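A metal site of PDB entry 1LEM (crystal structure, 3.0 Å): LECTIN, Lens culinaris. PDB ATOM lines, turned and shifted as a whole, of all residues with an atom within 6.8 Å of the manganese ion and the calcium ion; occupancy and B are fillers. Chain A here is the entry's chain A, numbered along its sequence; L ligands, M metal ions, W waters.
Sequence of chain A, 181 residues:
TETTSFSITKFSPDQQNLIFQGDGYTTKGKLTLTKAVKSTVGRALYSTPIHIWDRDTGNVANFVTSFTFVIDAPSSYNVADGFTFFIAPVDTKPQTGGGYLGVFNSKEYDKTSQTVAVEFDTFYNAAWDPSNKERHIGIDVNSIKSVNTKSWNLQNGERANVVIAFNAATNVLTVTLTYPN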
ATOM      1  N   ASP A  81      -6.809  -0.132   3.379  1.00  0.00           N
ATOM      2  CA  ASP A  81      -6.165  -0.517   4.587  1.00  0.00           C
ATOM      3  C   ASP A  81      -6.083  -1.951   4.992  1.00  0.00           C
ATOM      4  O   ASP A  81      -5.323  -2.305   5.923  1.00  0.00           O
ATOM      5  CB  ASP A  81      -6.900   0.178   5.726  1.00  0.00           C
ATOM      6  CG  ASP A  81      -6.113   1.341   6.309  1.00  0.00           C
ATOM      7  OD1 ASP A  81      -5.047   1.124   6.986  1.00  0.00           O
ATOM      8  OD2 ASP A  81      -6.527   2.549   6.119  1.00  0.00           O
ATOM      9  N   GLY A  98      -9.720   2.402  10.056  1.00  0.00           N
ATOM     10  CA  GLY A  98      -8.362   2.528   9.541  1.00  0.00           C
ATOM     11  C   GLY A  98      -7.466   1.299   9.783  1.00  0.00           C
ATOM     12  O   GLY A  98      -7.885   0.182   9.533  1.00  0.00           O
ATOM     13  N   GLY A  99      -6.298   1.369  10.421  1.00  0.00           N
ATOM     14  CA  GLY A  99      -5.409   0.227  10.574  1.00  0.00           C
ATOM     15  C   GLY A  99      -5.936  -0.860  11.486  1.00  0.00           C
ATOM     16  O   GLY A  99      -5.254  -1.900  11.510  1.00  0.00           O
ATOM     17  N   TYR A 100      -7.040  -0.591  12.271  1.00  0.00           N
ATOM     18  CA  TYR A 100      -7.709  -1.535  13.186  1.00  0.00           C
ATOM     19  C   TYR A 100      -8.723  -2.434  12.457  1.00  0.00           C
ATOM     20  O   TYR A 100      -9.273  -3.407  13.007  1.00  0.00           O
ATOM     21  CB  TYR A 100      -8.432  -0.790  14.312  1.00  0.00           C
ATOM     22  CG  TYR A 100      -7.474  -0.218  15.336  1.00  0.00           C
ATOM     23  CD1 TYR A 100      -6.700  -1.067  16.136  1.00  0.00           C
ATOM     24  CD2 TYR A 100      -7.344   1.152  15.471  1.00  0.00           C
ATOM     25  CE1 TYR A 100      -5.804  -0.543  17.060  1.00  0.00           C
ATOM     26  CE2 TYR A 100      -6.441   1.693  16.395  1.00  0.00           C
ATOM     27  CZ  TYR A 100      -5.662   0.854  17.203  1.00  0.00           C
ATOM     28  OH  TYR A 100      -4.766   1.392  18.147  1.00  0.00           O
ATOM     29  N   LEU A 101      -8.953  -2.062  11.165  1.00  0.00           N
ATOM     30  CA  LEU A 101      -9.641  -2.834  10.130  1.00  0.00           C
ATOM     31  C   LEU A 101     -11.080  -3.103  10.456  1.00  0.00           C
ATOM     32  O   LEU A 101     -11.626  -4.133  10.018  1.00  0.00           O
ATOM     33  CB  LEU A 101      -8.892  -4.171   9.920  1.00  0.00           C
ATOM     34  CG  LEU A 101      -7.473  -4.155   9.449  1.00  0.00           C
ATOM     35  CD1 LEU A 101      -6.949  -5.546   9.208  1.00  0.00           C
ATOM     36  CD2 LEU A 101      -7.438  -3.403   8.141  1.00  0.00           C
ATOM     37  N   GLU A 119      -6.354 -11.609   8.592  1.00  0.00           N
ATOM     38  CA  GLU A 119      -6.293 -10.341   7.904  1.00  0.00           C
ATOM     39  C   GLU A 119      -5.323 -10.403   6.743  1.00  0.00           C
ATOM     40  O   GLU A 119      -4.433 -11.269   6.644  1.00  0.00           O
ATOM     41  CB  GLU A 119      -5.875  -9.271   8.893  1.00  0.00           C
ATOM     42  CG  GLU A 119      -4.744  -9.753   9.839  1.00  0.00           C
ATOM     43  CD  GLU A 119      -3.886  -8.699  10.539  1.00  0.00           C
ATOM     44  OE1 GLU A 119      -4.363  -7.920  11.384  1.00  0.00           O
ATOM     45  OE2 GLU A 119      -2.689  -8.706  10.264  1.00  0.00           O
ATOM     46  N   ASP A 121      -3.428  -7.472   5.339  1.00  0.00           N
ATOM     47  CA  ASP A 121      -3.024  -6.102   5.704  1.00  0.00           C
ATOM     48  C   ASP A 121      -2.135  -5.468   4.664  1.00  0.00           C
ATOM     49  O   ASP A 121      -1.054  -6.031   4.380  1.00  0.00           O
ATOM     50  CB  ASP A 121      -2.279  -6.062   7.024  1.00  0.00           C
ATOM     51  CG  ASP A 121      -2.129  -4.644   7.651  1.00  0.00           C
ATOM     52  OD1 ASP A 121      -2.400  -3.609   7.017  1.00  0.00           O
ATOM     53  OD2 ASP A 121      -1.789  -4.592   8.827  1.00  0.00           O
ATOM     54  N   THR A 122      -2.563  -4.289   4.212  1.00  0.00           N
ATOM     55  CA  THR A 122      -1.916  -3.650   3.070  1.00  0.00           C
ATOM     56  C   THR A 122      -1.160  -2.401   3.440  1.00  0.00           C
ATOM     57  O   THR A 122      -0.624  -1.676   2.592  1.00  0.00           O
ATOM     58  CB  THR A 122      -2.926  -3.226   1.875  1.00  0.00           C
ATOM     59  OG1 THR A 122      -4.039  -2.473   2.386  1.00  0.00           O
ATOM     60  CG2 THR A 122      -3.390  -4.438   1.087  1.00  0.00           C
ATOM     61  N   PHE A 123      -1.097  -2.179   4.739  1.00  0.00           N
ATOM     62  CA  PHE A 123      -0.516  -0.943   5.220  1.00  0.00           C
ATOM     63  C   PHE A 123       0.056  -1.106   6.612  1.00  0.00           C
ATOM     64  O   PHE A 123      -0.669  -1.561   7.527  1.00  0.00           O
ATOM     65  CB  PHE A 123      -1.634   0.020   5.159  1.00  0.00           C
ATOM     66  CG  PHE A 123      -1.182   1.360   5.571  1.00  0.00           C
ATOM     67  CD1 PHE A 123      -0.694   2.180   4.587  1.00  0.00           C
ATOM     68  CD2 PHE A 123      -1.322   1.781   6.877  1.00  0.00           C
ATOM     69  CE1 PHE A 123      -0.321   3.461   4.926  1.00  0.00           C
ATOM     70  CE2 PHE A 123      -0.943   3.060   7.203  1.00  0.00           C
ATOM     71  CZ  PHE A 123      -0.454   3.899   6.231  1.00  0.00           C
ATOM     72  N   TYR A 124       1.376  -0.713   6.701  1.00  0.00           N
ATOM     73  CA  TYR A 124       2.151  -0.805   7.950  1.00  0.00           C
ATOM     74  C   TYR A 124       1.801   0.302   8.944  1.00  0.00           C
ATOM     75  O   TYR A 124       1.921   1.522   8.750  1.00  0.00           O
ATOM     76  CB  TYR A 124       3.736  -0.767   7.686  1.00  0.00           C
ATOM     77  CG  TYR A 124       4.754  -0.809   8.880  1.00  0.00           C
ATOM     78  CD1 TYR A 124       5.055  -1.996   9.562  1.00  0.00           C
ATOM     79  CD2 TYR A 124       5.419   0.361   9.330  1.00  0.00           C
ATOM     80  CE1 TYR A 124       5.984  -2.021  10.611  1.00  0.00           C
ATOM     81  CE2 TYR A 124       6.350   0.342  10.372  1.00  0.00           C
ATOM     82  CZ  TYR A 124       6.615  -0.851  11.033  1.00  0.00           C
ATOM     83  OH  TYR A 124       7.496  -0.893  12.113  1.00  0.00           O
ATOM     84  N   ASN A 125       1.383  -0.223  10.083  1.00  0.00           N
ATOM     85  CA  ASN A 125       1.037   0.584  11.205  1.00  0.00           C
ATOM     86  C   ASN A 125       2.193   0.152  12.065  1.00  0.00           C
ATOM     87  O   ASN A 125       2.415  -0.996  12.486  1.00  0.00           O
ATOM     88  CB  ASN A 125      -0.294   0.143  11.721  1.00  0.00           C
ATOM     89  CG  ASN A 125      -1.432   0.484  10.754  1.00  0.00           C
ATOM     90  OD1 ASN A 125      -1.949  -0.298   9.941  1.00  0.00           O
ATOM     91  ND2 ASN A 125      -1.812   1.741  10.914  1.00  0.00           N
ATOM     92  N   TRP A 128       2.356  -1.785  15.524  1.00  0.00           N
ATOM     93  CA  TRP A 128       1.976  -3.184  15.805  1.00  0.00           C
ATOM     94  C   TRP A 128       2.260  -4.117  14.653  1.00  0.00           C
ATOM     95  O   TRP A 128       2.277  -5.348  14.809  1.00  0.00           O
ATOM     96  CB  TRP A 128       0.449  -3.349  16.139  1.00  0.00           C
ATOM     97  CG  TRP A 128      -0.589  -2.788  15.138  1.00  0.00           C
ATOM     98  CD1 TRP A 128      -0.749  -3.319  13.876  1.00  0.00           C
ATOM     99  CD2 TRP A 128      -1.376  -1.673  15.330  1.00  0.00           C
ATOM    100  NE1 TRP A 128      -1.594  -2.529  13.245  1.00  0.00           N
ATOM    101  CE2 TRP A 128      -1.980  -1.518  14.073  1.00  0.00           C
ATOM    102  CE3 TRP A 128      -1.656  -0.755  16.317  1.00  0.00           C
ATOM    103  CZ2 TRP A 128      -2.865  -0.481  13.803  1.00  0.00           C
ATOM    104  CZ3 TRP A 128      -2.540   0.287  16.039  1.00  0.00           C
ATOM    105  CH2 TRP A 128      -3.146   0.432  14.799  1.00  0.00           C
ATOM    106  N   ASP A 129       2.421  -3.547  13.459  1.00  0.00           N
ATOM    107  CA  ASP A 129       2.576  -4.398  12.295  1.00  0.00           C
ATOM    108  C   ASP A 129       4.036  -4.793  12.234  1.00  0.00           C
ATOM    109  O   ASP A 129       4.877  -4.026  12.744  1.00  0.00           O
ATOM    110  CB  ASP A 129       2.100  -3.642  11.005  1.00  0.00           C
ATOM    111  CG  ASP A 129       0.578  -3.708  10.706  1.00  0.00           C
ATOM    112  OD1 ASP A 129      -0.096  -4.656  11.111  1.00  0.00           O
ATOM    113  OD2 ASP A 129       0.034  -2.814  10.063  1.00  0.00           O
ATOM    114  N   PRO A 130       4.404  -5.948  11.657  1.00  0.00           N
ATOM    115  CA  PRO A 130       5.778  -6.407  11.483  1.00  0.00           C
ATOM    116  C   PRO A 130       6.700  -5.324  10.971  1.00  0.00           C
ATOM    117  O   PRO A 130       6.511  -4.756   9.873  1.00  0.00           O
ATOM    118  CB  PRO A 130       5.815  -7.527  10.487  1.00  0.00           C
ATOM    119  CG  PRO A 130       4.407  -8.017  10.551  1.00  0.00           C
ATOM    120  CD  PRO A 130       3.598  -6.744  10.735  1.00  0.00           C
ATOM    121  N   HIS A 136       1.134  -8.454   4.495  1.00  0.00           N
ATOM    122  CA  HIS A 136       1.086  -9.728   5.181  1.00  0.00           C
ATOM    123  C   HIS A 136      -0.295 -10.270   5.444  1.00  0.00           C
ATOM    124  O   HIS A 136      -1.267  -9.490   5.535  1.00  0.00           O
ATOM    125  CB  HIS A 136       1.850  -9.559   6.492  1.00  0.00           C
ATOM    126  CG  HIS A 136       1.298  -8.414   7.338  1.00  0.00           C
ATOM    127  ND1 HIS A 136       1.589  -7.116   7.219  1.00  0.00           N
ATOM    128  CD2 HIS A 136       0.390  -8.530   8.403  1.00  0.00           C
ATOM    129  CE1 HIS A 136       0.907  -6.470   8.141  1.00  0.00           C
ATOM    130  NE2 HIS A 136       0.185  -7.313   8.862  1.00  0.00           N
ATOM    131  N   GLY A 138      -2.208 -12.274   8.358  1.00  0.00           N
ATOM    132  CA  GLY A 138      -1.993 -12.474   9.773  1.00  0.00           C
ATOM    133  C   GLY A 138      -3.234 -13.133  10.412  1.00  0.00           C
ATOM    134  O   GLY A 138      -4.362 -12.972   9.907  1.00  0.00           O
ATOM    135  N   ASP A 140      -5.188 -13.042  14.060  1.00  0.00           N
ATOM    136  CA  ASP A 140      -5.199 -12.253  15.275  1.00  0.00           C
ATOM    137  C   ASP A 140      -6.300 -12.772  16.158  1.00  0.00           C
ATOM    138  O   ASP A 140      -7.401 -13.178  15.717  1.00  0.00           O
ATOM    139  CB  ASP A 140      -5.629 -10.862  15.167  1.00  0.00           C
ATOM    140  CG  ASP A 140      -5.368 -10.232  13.847  1.00  0.00           C
ATOM    141  OD1 ASP A 140      -4.466 -10.647  13.143  1.00  0.00           O
ATOM    142  OD2 ASP A 140      -6.086  -9.300  13.530  1.00  0.00           O
ATOM    143  N   ILE A 144      -5.478  -6.238  17.625  1.00  0.00           N
ATOM    144  CA  ILE A 144      -4.974  -5.935  16.291  1.00  0.00           C
ATOM    145  C   ILE A 144      -3.535  -6.380  15.977  1.00  0.00           C
ATOM    146  O   ILE A 144      -3.049  -6.280  14.845  1.00  0.00           O
ATOM    147  CB  ILE A 144      -5.112  -4.441  16.037  1.00  0.00           C
ATOM    148  CG1 ILE A 144      -5.033  -4.162  14.521  1.00  0.00           C
ATOM    149  CG2 ILE A 144      -4.013  -3.707  16.754  1.00  0.00           C
ATOM    150  CD1 ILE A 144      -6.158  -4.683  13.592  1.00  0.00           C
ATOM    151  N   LYS A 145      -2.798  -6.852  16.984  1.00  0.00           N
ATOM    152  CA  LYS A 145      -1.459  -7.407  16.837  1.00  0.00           C
ATOM    153  C   LYS A 145      -1.446  -8.881  16.461  1.00  0.00           C
ATOM    154  O   LYS A 145      -1.672  -9.722  17.335  1.00  0.00           O
ATOM    155  CB  LYS A 145      -0.761  -7.218  18.165  1.00  0.00           C
ATOM    156  CG  LYS A 145       0.382  -6.218  18.147  1.00  0.00           C
ATOM    157  CD  LYS A 145       1.689  -6.944  17.920  1.00  0.00           C
ATOM    158  CE  LYS A 145       2.020  -7.591  19.250  1.00  0.00           C
ATOM    159  NZ  LYS A 145       2.511  -8.954  19.083  1.00  0.00           N
ATOM    160  N   SER A 146      -1.217  -9.273  15.223  1.00  0.00           N
ATOM    161  CA  SER A 146      -1.281 -10.683  14.890  1.00  0.00           C
ATOM    162  C   SER A 146      -0.412 -11.580  15.743  1.00  0.00           C
ATOM    163  O   SER A 146       0.733 -11.271  16.042  1.00  0.00           O
ATOM    164  CB  SER A 146      -0.860 -10.959  13.465  1.00  0.00           C
ATOM    165  OG  SER A 146      -1.154  -9.828  12.650  1.00  0.00           O
ATOM    166  N   THR A 149       2.150 -14.167  11.429  1.00  0.00           N
ATOM    167  CA  THR A 149       2.043 -13.508  10.137  1.00  0.00           C
ATOM    168  C   THR A 149       2.861 -14.264   9.065  1.00  0.00           C
ATOM    169  O   THR A 149       3.687 -15.165   9.356  1.00  0.00           O
ATOM    170  CB  THR A 149       2.541 -12.008  10.167  1.00  0.00           C
ATOM    171  OG1 THR A 149       3.835 -12.149  10.648  1.00  0.00           O
ATOM    172  CG2 THR A 149       1.875 -10.995  11.079  1.00  0.00           C
HETATM  173  C1  LIG L   1      -4.751   7.004   8.975  1.00  0.00           C
HETATM  174  C2  LIG L   1      -5.396   6.082  10.064  1.00  0.00           C
HETATM  175  C3  LIG L   1      -4.616   4.707  10.158  1.00  0.00           C
HETATM  176  C4  LIG L   1      -4.590   4.043   8.786  1.00  0.00           C
HETATM  177  C5  LIG L   1      -3.867   4.924   7.765  1.00  0.00           C
HETATM  178  C6  LIG L   1      -3.856   4.341   6.264  1.00  0.00           C
HETATM  179  O1  LIG L   1      -3.478   7.447   9.560  1.00  0.00           O
HETATM  180  O2  LIG L   1      -5.249   6.736  11.321  1.00  0.00           O
HETATM  181  O3  LIG L   1      -5.122   3.801  11.144  1.00  0.00           O
HETATM  182  O4  LIG L   1      -3.921   2.819   8.916  1.00  0.00           O
HETATM  183  O5  LIG L   1      -4.526   6.229   7.762  1.00  0.00           O
HETATM  184  O6  LIG L   1      -4.945   4.742   5.427  1.00  0.00           O
HETATM  185 MN    MN M   1      -1.285  -6.318  10.568  1.00  0.00          MN
HETATM  186 CA    CA M   2      -2.325  -2.291   9.352  1.00  0.00          CA
HETATM  187  O   HOH W   1       0.510  -7.725  12.585  1.00  0.00           O
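ND2 of Asn 125 lies within hydrogen-bond range of O4 of the ligand, 3.1 Å away. N of Gly 99 lies within hydrogen-bond range of O3 of the ligand, at 2.8 Å. OD2 of Asp 81 sits at hydrogen-bond distance from O6 of the ligand, 2.8 Å away.
Gly 99 touches the calcium ion (O to CA, 3.7 Å). Trp 128 touches the calcium ion. The nearest printed residue that does not touch the calcium ion is Asp 81 (4.6 Å).
OD1 of Asp 129 lies close to NE1 of Trp 128, 3.4 Å away. A ring nitrogen (NE2) of His 136 sits close to the side-chain carboxylate (OE2) of Glu 119 (3.5 Å). OG of Ser 146 is in hydrogen-bond range of OE2 of Glu 119, 3.1 Å away. The backbone NH (N) of Glu 119 lies within hydrogen-bond range of the backbone carbonyl oxygen (O) of Gly 138, 2.7 Å away.
The manganese ion is bound by OD1 of Asp 129 (2.1 Å), NE2 of His 136 (2.5 Å) and OD2 of Asp 121 (2.5 Å). The manganese ion has three donor atoms within binding distance. Slightly farther from the manganese ion lies OE2 of Glu 119 (2.8 Å).
Within 4 Å of the manganese ion: Glu 119, Asp 121, Asp 129 and His 136. The nearest printed residue that does not touch the manganese ion is Ser 146 (4.1 Å).
The calcium ion is bound by the side-chain amide oxygen (OD1) of Asn 125 (2.1 Å), the side-chain carboxylate (OD2) of Asp 121 (2.4 Å), the side-chain carboxylate (OD2) of Asp 129 (2.5 Å), the backbone carbonyl oxygen (O) of Phe 123 (2.6 Å) and the side-chain carboxylate (OD1) of Asp 121 (2.7 Å).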
